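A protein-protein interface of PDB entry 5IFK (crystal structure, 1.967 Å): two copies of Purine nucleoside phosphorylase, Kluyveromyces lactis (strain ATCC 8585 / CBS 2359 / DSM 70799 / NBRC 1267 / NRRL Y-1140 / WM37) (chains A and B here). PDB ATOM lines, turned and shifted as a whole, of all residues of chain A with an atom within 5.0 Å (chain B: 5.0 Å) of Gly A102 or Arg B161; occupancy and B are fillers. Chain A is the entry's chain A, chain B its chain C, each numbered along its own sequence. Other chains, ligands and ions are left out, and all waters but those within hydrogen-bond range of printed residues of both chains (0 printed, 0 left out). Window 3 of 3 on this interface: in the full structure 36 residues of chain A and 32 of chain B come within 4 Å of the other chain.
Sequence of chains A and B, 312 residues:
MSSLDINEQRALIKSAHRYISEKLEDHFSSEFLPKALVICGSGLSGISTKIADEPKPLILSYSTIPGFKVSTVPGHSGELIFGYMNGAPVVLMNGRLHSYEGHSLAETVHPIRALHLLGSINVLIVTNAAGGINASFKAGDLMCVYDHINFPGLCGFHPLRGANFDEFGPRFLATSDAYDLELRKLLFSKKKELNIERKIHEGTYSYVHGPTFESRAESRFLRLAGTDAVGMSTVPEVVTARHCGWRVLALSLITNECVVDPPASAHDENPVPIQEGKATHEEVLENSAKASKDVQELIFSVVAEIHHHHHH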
ATOM      1  N   HIS A  98       5.717  31.492  14.618  1.00  0.00           N
ATOM      2  CA  HIS A  98       5.610  30.481  15.676  1.00  0.00           C
ATOM      3  C   HIS A  98       6.813  30.481  16.621  1.00  0.00           C
ATOM      4  O   HIS A  98       7.957  30.544  16.177  1.00  0.00           O
ATOM      5  CB  HIS A  98       5.457  29.086  15.068  1.00  0.00           C
ATOM      6  CG  HIS A  98       4.226  28.919  14.234  1.00  0.00           C
ATOM      7  ND1 HIS A  98       2.967  28.809  14.783  1.00  0.00           N
ATOM      8  CD2 HIS A  98       4.062  28.836  12.893  1.00  0.00           C
ATOM      9  CE1 HIS A  98       2.077  28.677  13.816  1.00  0.00           C
ATOM     10  NE2 HIS A  98       2.717  28.689  12.658  1.00  0.00           N
ATOM     11  N   SER A  99       6.547  30.385  17.922  1.00  0.00           N
ATOM     12  CA  SER A  99       7.603  30.361  18.943  1.00  0.00           C
ATOM     13  C   SER A  99       8.594  29.222  18.766  1.00  0.00           C
ATOM     14  O   SER A  99       9.782  29.390  19.028  1.00  0.00           O
ATOM     15  CB  SER A  99       6.992  30.251  20.334  1.00  0.00           C
ATOM     16  OG  SER A  99       6.128  31.336  20.571  1.00  0.00           O
ATOM     17  N   TYR A 100       8.117  28.055  18.326  1.00  0.00           N
ATOM     18  CA  TYR A 100       9.017  26.906  18.203  1.00  0.00           C
ATOM     19  C   TYR A 100      10.041  27.154  17.108  1.00  0.00           C
ATOM     20  O   TYR A 100      11.053  26.457  17.027  1.00  0.00           O
ATOM     21  CB  TYR A 100       8.251  25.607  17.932  1.00  0.00           C
ATOM     22  CG  TYR A 100       7.314  25.635  16.742  1.00  0.00           C
ATOM     23  CD1 TYR A 100       7.795  25.539  15.437  1.00  0.00           C
ATOM     24  CD2 TYR A 100       5.943  25.716  16.929  1.00  0.00           C
ATOM     25  CE1 TYR A 100       6.920  25.548  14.349  1.00  0.00           C
ATOM     26  CE2 TYR A 100       5.072  25.736  15.863  1.00  0.00           C
ATOM     27  CZ  TYR A 100       5.560  25.651  14.577  1.00  0.00           C
ATOM     28  OH  TYR A 100       4.671  25.665  13.525  1.00  0.00           O
ATOM     29  N   GLU A 101       9.789  28.159  16.275  1.00  0.00           N
ATOM     30  CA  GLU A 101      10.758  28.523  15.244  1.00  0.00           C
ATOM     31  C   GLU A 101      11.879  29.376  15.827  1.00  0.00           C
ATOM     32  O   GLU A 101      12.879  29.629  15.154  1.00  0.00           O
ATOM     33  CB  GLU A 101      10.079  29.257  14.082  1.00  0.00           C
ATOM     34  CG  GLU A 101       9.314  28.323  13.148  1.00  0.00           C
ATOM     35  CD  GLU A 101      10.238  27.440  12.305  1.00  0.00           C
ATOM     36  OE1 GLU A 101      11.449  27.754  12.192  1.00  0.00           O
ATOM     37  OE2 GLU A 101       9.760  26.418  11.759  1.00  0.00           O
ATOM     38  N   GLY A 102      11.721  29.804  17.079  1.00  0.00           N
ATOM     39  CA  GLY A 102      12.759  30.584  17.728  1.00  0.00           C
ATOM     40  C   GLY A 102      12.421  32.046  17.980  1.00  0.00           C
ATOM     41  O   GLY A 102      13.195  32.757  18.617  1.00  0.00           O
ATOM     42  N   HIS A 103      11.269  32.504  17.494  1.00  0.00           N
ATOM     43  CA  HIS A 103      10.876  33.895  17.702  1.00  0.00           C
ATOM     44  C   HIS A 103      10.428  34.151  19.140  1.00  0.00           C
ATOM     45  O   HIS A 103       9.823  33.279  19.771  1.00  0.00           O
ATOM     46  CB  HIS A 103       9.740  34.287  16.755  1.00  0.00           C
ATOM     47  CG  HIS A 103       9.962  33.867  15.339  1.00  0.00           C
ATOM     48  ND1 HIS A 103      10.933  34.430  14.543  1.00  0.00           N
ATOM     49  CD2 HIS A 103       9.333  32.944  14.574  1.00  0.00           C
ATOM     50  CE1 HIS A 103      10.899  33.867  13.348  1.00  0.00           C
ATOM     51  NE2 HIS A 103       9.933  32.963  13.339  1.00  0.00           N
ATOM     52  N   SER A 104      10.708  35.351  19.646  1.00  0.00           N
ATOM     53  CA  SER A 104      10.176  35.769  20.937  1.00  0.00           C
ATOM     54  C   SER A 104       8.673  35.950  20.818  1.00  0.00           C
ATOM     55  O   SER A 104       8.152  36.151  19.712  1.00  0.00           O
ATOM     56  CB  SER A 104      10.827  37.070  21.405  1.00  0.00           C
ATOM     57  OG  SER A 104      10.399  38.159  20.610  1.00  0.00           O
ATOM     58  N   GLU A 107       7.827  39.277  19.346  1.00  0.00           N
ATOM     59  CA  GLU A 107       7.865  39.270  17.893  1.00  0.00           C
ATOM     60  C   GLU A 107       6.589  38.653  17.324  1.00  0.00           C
ATOM     61  O   GLU A 107       6.028  39.153  16.352  1.00  0.00           O
ATOM     62  CB  GLU A 107       9.112  38.528  17.405  1.00  0.00           C
ATOM     63  CG  GLU A 107      10.395  39.337  17.652  1.00  0.00           C
ATOM     64  CD  GLU A 107      11.673  38.515  17.579  1.00  0.00           C
ATOM     65  OE1 GLU A 107      11.608  37.263  17.659  1.00  0.00           O
ATOM     66  OE2 GLU A 107      12.750  39.138  17.452  1.00  0.00           O
ATOM     67  N   PHE A 157       7.025  31.800  29.923  1.00  0.00           N
ATOM     68  CA  PHE A 157       7.004  32.063  28.483  1.00  0.00           C
ATOM     69  C   PHE A 157       5.666  32.724  28.136  1.00  0.00           C
ATOM     70  O   PHE A 157       4.723  32.052  27.705  1.00  0.00           O
ATOM     71  CB  PHE A 157       7.207  30.754  27.713  1.00  0.00           C
ATOM     72  CG  PHE A 157       7.453  30.932  26.243  1.00  0.00           C
ATOM     73  CD1 PHE A 157       8.619  31.527  25.786  1.00  0.00           C
ATOM     74  CD2 PHE A 157       6.526  30.471  25.314  1.00  0.00           C
ATOM     75  CE1 PHE A 157       8.850  31.685  24.422  1.00  0.00           C
ATOM     76  CE2 PHE A 157       6.751  30.616  23.960  1.00  0.00           C
ATOM     77  CZ  PHE A 157       7.923  31.231  23.514  1.00  0.00           C
ATOM     78  N   HIS A 209       4.356  24.419  23.672  1.00  0.00           N
ATOM     79  CA  HIS A 209       5.347  25.073  22.813  1.00  0.00           C
ATOM     80  C   HIS A 209       5.640  24.336  21.487  1.00  0.00           C
ATOM     81  O   HIS A 209       5.817  24.974  20.439  1.00  0.00           O
ATOM     82  CB  HIS A 209       6.649  25.275  23.596  1.00  0.00           C
ATOM     83  CG  HIS A 209       7.693  26.029  22.834  1.00  0.00           C
ATOM     84  ND1 HIS A 209       8.617  25.397  22.031  1.00  0.00           N
ATOM     85  CD2 HIS A 209       7.960  27.355  22.747  1.00  0.00           C
ATOM     86  CE1 HIS A 209       9.420  26.301  21.496  1.00  0.00           C
ATOM     87  NE2 HIS A 209       9.036  27.501  21.907  1.00  0.00           N
ATOM     88  N   PRO A 211       8.210  21.876  19.084  1.00  0.00           N
ATOM     89  CA  PRO A 211       7.535  21.392  17.883  1.00  0.00           C
ATOM     90  C   PRO A 211       7.298  19.883  17.886  1.00  0.00           C
ATOM     91  O   PRO A 211       6.904  19.351  16.856  1.00  0.00           O
ATOM     92  CB  PRO A 211       8.519  21.766  16.775  1.00  0.00           C
ATOM     93  CG  PRO A 211       9.863  21.526  17.442  1.00  0.00           C
ATOM     94  CD  PRO A 211       9.676  21.899  18.907  1.00  0.00           C
ATOM     95  N   GLY B 156       8.636  25.614  26.477  1.00  0.00           N
ATOM     96  CA  GLY B 156       9.553  26.403  25.668  1.00  0.00           C
ATOM     97  C   GLY B 156      11.009  26.004  25.787  1.00  0.00           C
ATOM     98  O   GLY B 156      11.842  26.380  24.963  1.00  0.00           O
ATOM     99  N   HIS B 158      13.111  23.512  25.016  1.00  0.00           N
ATOM    100  CA  HIS B 158      12.991  22.354  24.131  1.00  0.00           C
ATOM    101  C   HIS B 158      14.231  22.254  23.240  1.00  0.00           C
ATOM    102  O   HIS B 158      14.648  23.257  22.658  1.00  0.00           O
ATOM    103  CB  HIS B 158      11.720  22.505  23.292  1.00  0.00           C
ATOM    104  CG  HIS B 158      11.237  21.239  22.659  1.00  0.00           C
ATOM    105  ND1 HIS B 158      11.938  20.586  21.669  1.00  0.00           N
ATOM    106  CD2 HIS B 158      10.095  20.532  22.842  1.00  0.00           C
ATOM    107  CE1 HIS B 158      11.265  19.513  21.289  1.00  0.00           C
ATOM    108  NE2 HIS B 158      10.142  19.458  21.983  1.00  0.00           N
ATOM    109  N   PRO B 159      14.845  21.054  23.146  1.00  0.00           N
ATOM    110  CA  PRO B 159      16.081  20.946  22.361  1.00  0.00           C
ATOM    111  C   PRO B 159      15.855  21.178  20.868  1.00  0.00           C
ATOM    112  O   PRO B 159      16.824  21.385  20.129  1.00  0.00           O
ATOM    113  CB  PRO B 159      16.541  19.502  22.622  1.00  0.00           C
ATOM    114  CG  PRO B 159      15.283  18.767  22.958  1.00  0.00           C
ATOM    115  CD  PRO B 159      14.463  19.762  23.748  1.00  0.00           C
ATOM    116  N   LEU B 160      14.600  21.146  20.424  1.00  0.00           N
ATOM    117  CA  LEU B 160      14.319  21.340  19.001  1.00  0.00           C
ATOM    118  C   LEU B 160      13.811  22.750  18.712  1.00  0.00           C
ATOM    119  O   LEU B 160      13.502  23.084  17.552  1.00  0.00           O
ATOM    120  CB  LEU B 160      13.303  20.303  18.490  1.00  0.00           C
ATOM    121  CG  LEU B 160      13.709  18.828  18.557  1.00  0.00           C
ATOM    122  CD1 LEU B 160      12.645  17.965  17.915  1.00  0.00           C
ATOM    123  CD2 LEU B 160      15.080  18.583  17.885  1.00  0.00           C
ATOM    124  N   ARG B 161      13.715  23.584  19.752  1.00  0.00           N
ATOM    125  CA  ARG B 161      13.303  24.974  19.526  1.00  0.00           C
ATOM    126  C   ARG B 161      14.298  25.659  18.584  1.00  0.00           C
ATOM    127  O   ARG B 161      15.507  25.449  18.703  1.00  0.00           O
ATOM    128  CB  ARG B 161      13.196  25.757  20.848  1.00  0.00           C
ATOM    129  CG  ARG B 161      12.824  27.217  20.631  1.00  0.00           C
ATOM    130  CD  ARG B 161      12.410  27.929  21.897  1.00  0.00           C
ATOM    131  NE  ARG B 161      11.644  29.133  21.575  1.00  0.00           N
ATOM    132  CZ  ARG B 161      12.067  30.374  21.784  1.00  0.00           C
ATOM    133  NH1 ARG B 161      13.243  30.596  22.355  1.00  0.00           N
ATOM    134  NH2 ARG B 161      11.298  31.398  21.443  1.00  0.00           N
ATOM    135  N   GLY B 162      13.793  26.459  17.644  1.00  0.00           N
ATOM    136  CA  GLY B 162      14.645  27.121  16.668  1.00  0.00           C
ATOM    137  C   GLY B 162      14.479  26.533  15.282  1.00  0.00           C
ATOM    138  O   GLY B 162      13.615  25.687  15.066  1.00  0.00           O
ATOM    139  N   ALA B 163      15.302  26.973  14.335  1.00  0.00           N
ATOM    140  CA  ALA B 163      15.240  26.438  12.979  1.00  0.00           C
ATOM    141  C   ALA B 163      15.498  24.936  13.019  1.00  0.00           C
ATOM    142  O   ALA B 163      16.385  24.459  13.752  1.00  0.00           O
ATOM    143  CB  ALA B 163      16.254  27.132  12.065  1.00  0.00           C
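Hydrophobic or aromatic side chains of chain B within 4 Å of the printed part of chain A: His B158 and Leu B160. Of the 11 printed residues of chain A, 8 touch a printed residue of chain B. Hydrophobic or aromatic side chains of chain A that line the printed part of chain B: Phe A157, His A209 and Pro A211. Among the printed residues, no Asp or Glu carboxylate lies within 4 Å of a Lys or Arg side-chain nitrogen of the other chain.
No position is printed for both chains. Of the 13 pairs that touch across the chains among the printed residues, none has its exchanged pair printed and touching as well.
Of the printed residues of chain B, Glu A101 touches Gly B162 and Ala B163. Of chain B, only Arg B161 (3.7 Å) and Gly B162 (3.98 Å) come within 4 Å of Gly A102. Printed residues of chain A within 4 Å of Gly B156: His A209. Of the printed residues of chain A, His B158 touches Pro A211. Pro B159 touches none of the printed residues of chain A. Of the printed residues of chain A, Gly B162 touches Tyr A100 (2.8 Å), Glu A101 (3.4 Å) and Gly A102 (3.98 Å). Printed residues of chain A within 4 Å of Ala B163: Glu A101 (3.7 Å). The nearest printed residue of chain B that does not touch Gly A102 is Ala B163 (5.3 Å). The nearest residue of chain A that does not touch Arg B161 is Ser A104 (4.4 Å). The nearest printed residue of chain A that does not touch Gly B156 is Phe A157 (5.0 Å).
Among the printed residues, merely in contact across the chains: Tyr A100 with Arg B161, Glu A101 with Gly B162, Glu A101 with Ala B163, Gly A102 with Arg B161, Gly A102 with Gly B162, Phe A157 with Arg B161, His A209 with Gly B156, Pro A211 with His B158 and Pro A211 with Leu B160.
ND1 of His B158 is in hydrogen-bond range of N of Leu B160, at 3.0 Å.
NE2 of His A209 lies within hydrogen-bond range of NE of Arg B161, at 3.1 Å. The backbone carbonyl oxygen (O) of Tyr A100 sits at hydrogen-bond distance from the backbone NH (N) of Gly B162, at 2.8 Å. The backbone carbonyl oxygen of His A103 is in hydrogen-bond range of the guanidinium group of Arg B161, at 2.9 Å. The guanidinium group of Arg B161 sits at hydrogen-bond distance from the backbone carbonyl oxygen of Ser A99, at 3.2 Å.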
